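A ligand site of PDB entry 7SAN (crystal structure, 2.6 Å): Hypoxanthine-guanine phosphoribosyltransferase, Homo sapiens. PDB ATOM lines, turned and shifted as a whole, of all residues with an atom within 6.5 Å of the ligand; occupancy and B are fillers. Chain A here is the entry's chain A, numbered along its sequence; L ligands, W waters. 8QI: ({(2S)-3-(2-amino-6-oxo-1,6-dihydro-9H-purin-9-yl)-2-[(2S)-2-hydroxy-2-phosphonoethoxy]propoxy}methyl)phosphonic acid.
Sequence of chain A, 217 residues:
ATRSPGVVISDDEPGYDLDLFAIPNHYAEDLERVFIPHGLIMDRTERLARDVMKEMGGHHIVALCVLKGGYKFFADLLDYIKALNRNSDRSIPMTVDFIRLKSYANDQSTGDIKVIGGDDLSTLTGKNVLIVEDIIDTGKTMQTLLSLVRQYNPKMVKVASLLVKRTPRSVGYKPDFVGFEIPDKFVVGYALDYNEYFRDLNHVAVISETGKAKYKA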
ATOM      1  N   GLY A  69       1.300   1.411  -2.699  1.00  0.00           N
ATOM      2  CA  GLY A  69       2.345   0.418  -2.593  1.00  0.00           C
ATOM      3  C   GLY A  69       2.113  -0.726  -3.555  1.00  0.00           C
ATOM      4  O   GLY A  69       3.068  -1.339  -4.043  1.00  0.00           O
ATOM      5  N   GLU A 133      -2.137  -6.496   2.551  1.00  0.00           N
ATOM      6  CA  GLU A 133      -0.898  -5.746   2.341  1.00  0.00           C
ATOM      7  C   GLU A 133       0.040  -6.504   1.411  1.00  0.00           C
ATOM      8  O   GLU A 133       0.099  -7.734   1.440  1.00  0.00           O
ATOM      9  CB  GLU A 133      -0.227  -5.461   3.688  1.00  0.00           C
ATOM     10  CG  GLU A 133       1.071  -4.679   3.604  1.00  0.00           C
ATOM     11  CD  GLU A 133       0.867  -3.262   3.092  1.00  0.00           C
ATOM     12  OE1 GLU A 133      -0.276  -2.751   3.173  1.00  0.00           O
ATOM     13  OE2 GLU A 133       1.849  -2.655   2.616  1.00  0.00           O
ATOM     14  N   ASP A 134       0.791  -5.773   0.590  1.00  0.00           N
ATOM     15  CA  ASP A 134       1.700  -6.397  -0.369  1.00  0.00           C
ATOM     16  C   ASP A 134       3.040  -6.761   0.268  1.00  0.00           C
ATOM     17  O   ASP A 134       3.591  -7.825  -0.019  1.00  0.00           O
ATOM     18  CB  ASP A 134       1.914  -5.479  -1.573  1.00  0.00           C
ATOM     19  CG  ASP A 134       2.428  -4.106  -1.190  1.00  0.00           C
ATOM     20  OD1 ASP A 134       2.241  -3.707  -0.026  1.00  0.00           O
ATOM     21  OD2 ASP A 134       3.019  -3.425  -2.055  1.00  0.00           O
ATOM     22  N   ILE A 135       3.564  -5.891   1.120  1.00  0.00           N
ATOM     23  CA  ILE A 135       4.828  -6.171   1.801  1.00  0.00           C
ATOM     24  C   ILE A 135       4.896  -5.534   3.182  1.00  0.00           C
ATOM     25  O   ILE A 135       4.388  -4.435   3.411  1.00  0.00           O
ATOM     26  CB  ILE A 135       6.032  -5.685   0.944  1.00  0.00           C
ATOM     27  CG1 ILE A 135       7.352  -6.158   1.569  1.00  0.00           C
ATOM     28  CG2 ILE A 135       6.008  -4.181   0.774  1.00  0.00           C
ATOM     29  CD1 ILE A 135       8.586  -5.630   0.882  1.00  0.00           C
ATOM     30  N   ILE A 136       5.521  -6.247   4.117  1.00  0.00           N
ATOM     31  CA  ILE A 136       5.773  -5.723   5.449  1.00  0.00           C
ATOM     32  C   ILE A 136       7.258  -5.764   5.769  1.00  0.00           C
ATOM     33  O   ILE A 136       7.877  -6.829   5.778  1.00  0.00           O
ATOM     34  CB  ILE A 136       4.986  -6.502   6.512  1.00  0.00           C
ATOM     35  CG1 ILE A 136       3.494  -6.236   6.364  1.00  0.00           C
ATOM     36  CG2 ILE A 136       5.466  -6.127   7.916  1.00  0.00           C
ATOM     37  CD1 ILE A 136       2.657  -6.826   7.455  1.00  0.00           C
ATOM     38  N   ASP A 137       7.834  -4.589   6.004  1.00  0.00           N
ATOM     39  CA  ASP A 137       9.253  -4.478   6.293  1.00  0.00           C
ATOM     40  C   ASP A 137       9.492  -4.383   7.803  1.00  0.00           C
ATOM     41  O   ASP A 137       9.774  -5.386   8.448  1.00  0.00           O
ATOM     42  CB  ASP A 137       9.843  -3.268   5.566  1.00  0.00           C
ATOM     43  CG  ASP A 137      11.364  -3.209   5.655  1.00  0.00           C
ATOM     44  OD1 ASP A 137      11.983  -4.253   5.930  1.00  0.00           O
ATOM     45  OD2 ASP A 137      11.922  -2.121   5.429  1.00  0.00           O
ATOM     46  N   THR A 138       9.366  -3.181   8.348  1.00  0.00           N
ATOM     47  CA  THR A 138       9.538  -2.982   9.787  1.00  0.00           C
ATOM     48  C   THR A 138       8.263  -3.359  10.544  1.00  0.00           C
ATOM     49  O   THR A 138       8.318  -3.953  11.621  1.00  0.00           O
ATOM     50  CB  THR A 138       9.908  -1.527  10.120  1.00  0.00           C
ATOM     51  OG1 THR A 138       8.865  -0.650   9.691  1.00  0.00           O
ATOM     52  CG2 THR A 138      11.214  -1.137   9.435  1.00  0.00           C
ATOM     53  N   GLY A 139       7.113  -2.998   9.981  1.00  0.00           N
ATOM     54  CA  GLY A 139       5.836  -3.373  10.549  1.00  0.00           C
ATOM     55  C   GLY A 139       5.108  -2.257  11.281  1.00  0.00           C
ATOM     56  O   GLY A 139       3.981  -2.451  11.736  1.00  0.00           O
ATOM     57  N   LYS A 140       5.736  -1.092  11.382  1.00  0.00           N
ATOM     58  CA  LYS A 140       5.124   0.027  12.079  1.00  0.00           C
ATOM     59  C   LYS A 140       3.939   0.606  11.315  1.00  0.00           C
ATOM     60  O   LYS A 140       3.011   1.143  11.922  1.00  0.00           O
ATOM     61  CB  LYS A 140       6.148   1.136  12.352  1.00  0.00           C
ATOM     62  CG  LYS A 140       7.582   0.654  12.401  1.00  0.00           C
ATOM     63  CD  LYS A 140       8.548   1.833  12.411  1.00  0.00           C
ATOM     64  CE  LYS A 140       9.987   1.367  12.540  1.00  0.00           C
ATOM     65  NZ  LYS A 140      10.942   2.400  12.080  1.00  0.00           N
ATOM     66  N   THR A 141       3.979   0.509   9.992  1.00  0.00           N
ATOM     67  CA  THR A 141       2.862   0.958   9.170  1.00  0.00           C
ATOM     68  C   THR A 141       1.595   0.188   9.527  1.00  0.00           C
ATOM     69  O   THR A 141       0.510   0.768   9.651  1.00  0.00           O
ATOM     70  CB  THR A 141       3.148   0.784   7.663  1.00  0.00           C
ATOM     71  OG1 THR A 141       4.334   1.508   7.322  1.00  0.00           O
ATOM     72  CG2 THR A 141       1.986   1.288   6.829  1.00  0.00           C
ATOM     73  N   MET A 142       1.747  -1.120   9.717  1.00  0.00           N
ATOM     74  CA  MET A 142       0.607  -1.962  10.069  1.00  0.00           C
ATOM     75  C   MET A 142       0.173  -1.765  11.508  1.00  0.00           C
ATOM     76  O   MET A 142      -1.028  -1.714  11.795  1.00  0.00           O
ATOM     77  CB  MET A 142       0.937  -3.433   9.822  1.00  0.00           C
ATOM     78  CG  MET A 142       1.009  -3.812   8.350  1.00  0.00           C
ATOM     79  SD  MET A 142      -0.434  -3.285   7.407  1.00  0.00           S
ATOM     80  CE  MET A 142      -1.760  -3.976   8.397  1.00  0.00           C
ATOM     81  N   LYS A 165       9.660  -9.408   5.366  1.00  0.00           N
ATOM     82  CA  LYS A 165      11.119  -9.433   5.332  1.00  0.00           C
ATOM     83  C   LYS A 165      11.713  -9.721   6.702  1.00  0.00           C
ATOM     84  O   LYS A 165      11.293  -9.143   7.706  1.00  0.00           O
ATOM     85  CB  LYS A 165      11.654  -8.099   4.795  1.00  0.00           C
ATOM     86  CG  LYS A 165      11.137  -7.735   3.415  1.00  0.00           C
ATOM     87  CD  LYS A 165      11.654  -6.385   2.953  1.00  0.00           C
ATOM     88  CE  LYS A 165      13.170  -6.372   2.813  1.00  0.00           C
ATOM     89  NZ  LYS A 165      13.673  -5.070   2.301  1.00  0.00           N
ATOM     90  N   ILE A 182      11.089 -13.385   3.115  1.00  0.00           N
ATOM     91  CA  ILE A 182      12.236 -13.133   2.255  1.00  0.00           C
ATOM     92  C   ILE A 182      13.386 -12.436   2.985  1.00  0.00           C
ATOM     93  O   ILE A 182      13.170 -11.766   3.996  1.00  0.00           O
ATOM     94  CB  ILE A 182      11.828 -12.274   1.037  1.00  0.00           C
ATOM     95  CG1 ILE A 182      11.227 -10.943   1.491  1.00  0.00           C
ATOM     96  CG2 ILE A 182      10.847 -13.036   0.158  1.00  0.00           C
ATOM     97  CD1 ILE A 182      10.834 -10.024   0.352  1.00  0.00           C
ATOM     98  N   LYS A 185      16.482  -7.903   1.391  1.00  0.00           N
ATOM     99  CA  LYS A 185      16.894  -7.349   0.108  1.00  0.00           C
ATOM    100  C   LYS A 185      15.757  -6.527  -0.483  1.00  0.00           C
ATOM    101  O   LYS A 185      14.590  -6.854  -0.294  1.00  0.00           O
ATOM    102  CB  LYS A 185      17.293  -8.474  -0.850  1.00  0.00           C
ATOM    103  CG  LYS A 185      18.538  -9.238  -0.444  1.00  0.00           C
ATOM    104  CD  LYS A 185      19.788  -8.389  -0.644  1.00  0.00           C
ATOM    105  CE  LYS A 185      21.049  -9.203  -0.405  1.00  0.00           C
ATOM    106  NZ  LYS A 185      22.272  -8.423  -0.714  1.00  0.00           N
ATOM    107  N   PHE A 186      16.106  -5.457  -1.177  1.00  0.00           N
ATOM    108  CA  PHE A 186      15.080  -4.620  -1.796  1.00  0.00           C
ATOM    109  C   PHE A 186      14.555  -5.297  -3.058  1.00  0.00           C
ATOM    110  O   PHE A 186      15.271  -5.470  -4.036  1.00  0.00           O
ATOM    111  CB  PHE A 186      15.629  -3.235  -2.123  1.00  0.00           C
ATOM    112  CG  PHE A 186      14.567  -2.207  -2.358  1.00  0.00           C
ATOM    113  CD1 PHE A 186      14.016  -1.513  -1.301  1.00  0.00           C
ATOM    114  CD2 PHE A 186      14.089  -1.956  -3.636  1.00  0.00           C
ATOM    115  CE1 PHE A 186      13.023  -0.570  -1.508  1.00  0.00           C
ATOM    116  CE2 PHE A 186      13.093  -1.018  -3.851  1.00  0.00           C
ATOM    117  CZ  PHE A 186      12.561  -0.331  -2.783  1.00  0.00           C
ATOM    118  N   VAL A 187      13.274  -5.683  -3.019  1.00  0.00           N
ATOM    119  CA  VAL A 187      12.679  -6.429  -4.118  1.00  0.00           C
ATOM    120  C   VAL A 187      11.664  -5.613  -4.899  1.00  0.00           C
ATOM    121  O   VAL A 187      11.019  -4.715  -4.360  1.00  0.00           O
ATOM    122  CB  VAL A 187      11.986  -7.701  -3.596  1.00  0.00           C
ATOM    123  CG1 VAL A 187      13.018  -8.688  -3.059  1.00  0.00           C
ATOM    124  CG2 VAL A 187      10.964  -7.359  -2.525  1.00  0.00           C
ATOM    125  N   VAL A 188      11.540  -5.918  -6.192  1.00  0.00           N
ATOM    126  CA  VAL A 188      10.541  -5.298  -7.037  1.00  0.00           C
ATOM    127  C   VAL A 188       9.803  -6.365  -7.832  1.00  0.00           C
ATOM    128  O   VAL A 188      10.218  -7.528  -7.851  1.00  0.00           O
ATOM    129  CB  VAL A 188      11.166  -4.272  -8.019  1.00  0.00           C
ATOM    130  CG1 VAL A 188      11.761  -3.098  -7.253  1.00  0.00           C
ATOM    131  CG2 VAL A 188      12.215  -4.952  -8.881  1.00  0.00           C
ATOM    132  N   GLY A 189       8.700  -5.989  -8.480  1.00  0.00           N
ATOM    133  CA  GLY A 189       7.955  -6.913  -9.307  1.00  0.00           C
ATOM    134  C   GLY A 189       6.614  -7.330  -8.721  1.00  0.00           C
ATOM    135  O   GLY A 189       6.365  -7.146  -7.533  1.00  0.00           O
ATOM    136  N   LEU A 192       5.006  -4.772  -6.464  1.00  0.00           N
ATOM    137  CA  LEU A 192       5.927  -3.791  -5.886  1.00  0.00           C
ATOM    138  C   LEU A 192       6.712  -3.089  -6.980  1.00  0.00           C
ATOM    139  O   LEU A 192       7.290  -3.722  -7.855  1.00  0.00           O
ATOM    140  CB  LEU A 192       6.880  -4.470  -4.894  1.00  0.00           C
ATOM    141  CG  LEU A 192       6.313  -4.918  -3.541  1.00  0.00           C
ATOM    142  CD1 LEU A 192       5.534  -6.218  -3.635  1.00  0.00           C
ATOM    143  CD2 LEU A 192       7.432  -5.044  -2.524  1.00  0.00           C
ATOM    144  N   ASP A 193       6.735  -1.760  -6.919  1.00  0.00           N
ATOM    145  CA  ASP A 193       7.382  -0.946  -7.941  1.00  0.00           C
ATOM    146  C   ASP A 193       8.596  -0.201  -7.410  1.00  0.00           C
ATOM    147  O   ASP A 193       8.945  -0.305  -6.240  1.00  0.00           O
ATOM    148  CB  ASP A 193       6.379   0.059  -8.530  1.00  0.00           C
ATOM    149  CG  ASP A 193       5.889   1.060  -7.504  1.00  0.00           C
ATOM    150  OD1 ASP A 193       5.765   0.686  -6.318  1.00  0.00           O
ATOM    151  OD2 ASP A 193       5.634   2.215  -7.878  1.00  0.00           O
ATOM    152  N   TYR A 194       9.230   0.557  -8.301  1.00  0.00           N
ATOM    153  CA  TYR A 194      10.335   1.440  -7.932  1.00  0.00           C
ATOM    154  C   TYR A 194      10.228   2.711  -8.769  1.00  0.00           C
ATOM    155  O   TYR A 194      10.568   2.707  -9.950  1.00  0.00           O
ATOM    156  CB  TYR A 194      11.691   0.764  -8.138  1.00  0.00           C
ATOM    157  CG  TYR A 194      12.854   1.548  -7.592  1.00  0.00           C
ATOM    158  CD1 TYR A 194      13.589   2.408  -8.403  1.00  0.00           C
ATOM    159  CD2 TYR A 194      13.240   1.427  -6.261  1.00  0.00           C
ATOM    160  CE1 TYR A 194      14.657   3.127  -7.901  1.00  0.00           C
ATOM    161  CE2 TYR A 194      14.303   2.140  -5.752  1.00  0.00           C
ATOM    162  CZ  TYR A 194      15.011   2.996  -6.576  1.00  0.00           C
ATOM    163  OH  TYR A 194      16.071   3.703  -6.075  1.00  0.00           O
HETATM  164  C10 8QI L   1       7.254  -1.236   4.223  1.00  0.00           C
HETATM  165  C17 8QI L   1       6.874   1.562   2.571  1.00  0.00           C
HETATM  166  C24 8QI L   1       9.882  -1.543   2.125  1.00  0.00           C
HETATM  167  C26 8QI L   1      10.461  -2.664   0.380  1.00  0.00           C
HETATM  168  C02 8QI L   1       9.775  -2.389  -2.208  1.00  0.00           C
HETATM  169  C05 8QI L   1       9.591  -1.674  -0.008  1.00  0.00           C
HETATM  170  C07 8QI L   1       8.335   0.142   1.148  1.00  0.00           C
HETATM  171  C08 8QI L   1       7.753   0.323   2.551  1.00  0.00           C
HETATM  172  C11 8QI L   1       6.437  -0.385   5.179  1.00  0.00           C
HETATM  173  C19 8QI L   1       8.253   3.438   2.351  1.00  0.00           C
HETATM  174  C27 8QI L   1      10.984  -3.515  -0.607  1.00  0.00           C
HETATM  175  N01 8QI L   1       9.403  -2.237  -3.596  1.00  0.00           N
HETATM  176  N03 8QI L   1      10.623  -3.357  -1.870  1.00  0.00           N
HETATM  177  N04 8QI L   1       9.265  -1.567  -1.311  1.00  0.00           N
HETATM  178  N06 8QI L   1       9.250  -0.996   1.099  1.00  0.00           N
HETATM  179  N25 8QI L   1      10.625  -2.557   1.708  1.00  0.00           N
HETATM  180  O09 8QI L   1       7.003  -0.798   2.906  1.00  0.00           O
HETATM  181  O12 8QI L   1       5.078  -0.663   5.000  1.00  0.00           O
HETATM  182  O14 8QI L   1       8.427  -0.852   7.040  1.00  0.00           O
HETATM  183  O15 8QI L   1       6.333  -2.118   7.320  1.00  0.00           O
HETATM  184  O16 8QI L   1       6.410   0.276   7.870  1.00  0.00           O
HETATM  185  O18 8QI L   1       7.433   2.511   1.704  1.00  0.00           O
HETATM  186  O21 8QI L   1       8.768   4.613  -0.081  1.00  0.00           O
HETATM  187  O22 8QI L   1       9.219   5.984   1.916  1.00  0.00           O
HETATM  188  O23 8QI L   1       6.897   5.566   1.210  1.00  0.00           O
HETATM  189  O28 8QI L   1      11.874  -4.543  -0.263  1.00  0.00           O
HETATM  190  P13 8QI L   1       6.917  -0.791   6.931  1.00  0.00           P
HETATM  191  P20 8QI L   1       8.284   4.973   1.301  1.00  0.00           P
HETATM  192  O   HOH W   1      10.449  -0.035   5.525  1.00  0.00           O
HETATM  193  O   HOH W   2       7.550   2.468   8.499  1.00  0.00           O
HETATM  194  O   HOH W   3       4.038  -1.669   1.543  1.00  0.00           O
HETATM  195  O   HOH W   4       2.984  -2.522   5.247  1.00  0.00           O
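The side-chain amino group (NZ) of Lys 165 lies within hydrogen-bond range of the backbone carbonyl oxygen (O) of Lys 185 (3.3 Å). The backbone NH (N) of Lys 165 is in hydrogen-bond range of the backbone carbonyl oxygen (O) of Ile 136, 3.2 Å away.
Water W1 bridges the side-chain carboxylate of Asp 137 (2.6 Å) and an oxygen (O14) of the ligand (2.7 Å). Water W4 lies within hydrogen-bond range of an oxygen (O12) of the ligand (2.8 Å), the side-chain carboxylate of Glu 133 (2.9 Å) and the backbone carbonyl oxygen of Ile 135 (3.0 Å).
Residues that only touch the ligand: Ile 135 (3.5 Å), Lys 140 (3.8 Å), Lys 185 (3.6 Å), Phe 186 (3.5 Å) and Leu 192 (3.6 Å). Hydrophobic or aromatic side chains that line the ligand: Ile 135, Phe 186, Val 187 and Leu 192. Within 4 Å of the ligand: Ile 135, Asp 137, Thr 138, Gly 139, Lys 140, Thr 141, Lys 165, Lys 185, Phe 186, Val 187, Leu 192 and Asp 193.
The backbone NH (N) of Thr 141 is in hydrogen-bond range of an oxygen (O16) of the ligand (3.2 Å). O16 of the ligand sits at hydrogen-bond distance from OG1 of Thr 141. The backbone NH of Thr 138 is in hydrogen-bond range of an oxygen (O14) of the ligand, at 2.8 Å. The side-chain hydroxyl (OG1) of Thr 138 sits at hydrogen-bond distance from an oxygen (O14) of the ligand. O28 of the ligand lies within hydrogen-bond range of N of Val 187 (3.3 Å). A nitrogen (N03) of the ligand sits at hydrogen-bond distance from the backbone carbonyl oxygen (O) of Val 187 (2.9 Å). O15 of the ligand lies within hydrogen-bond range of N of Gly 139, at 2.9 Å. N of Asp 137 is in hydrogen-bond range of O15 of the ligand (3.2 Å). The side-chain amino group (NZ) of Lys 165 lies within hydrogen-bond range of an oxygen (O28) of the ligand, 3.2 Å away. A nitrogen (N01) of the ligand is in hydrogen-bond range of the backbone carbonyl oxygen of Asp 193 (3.3 Å).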
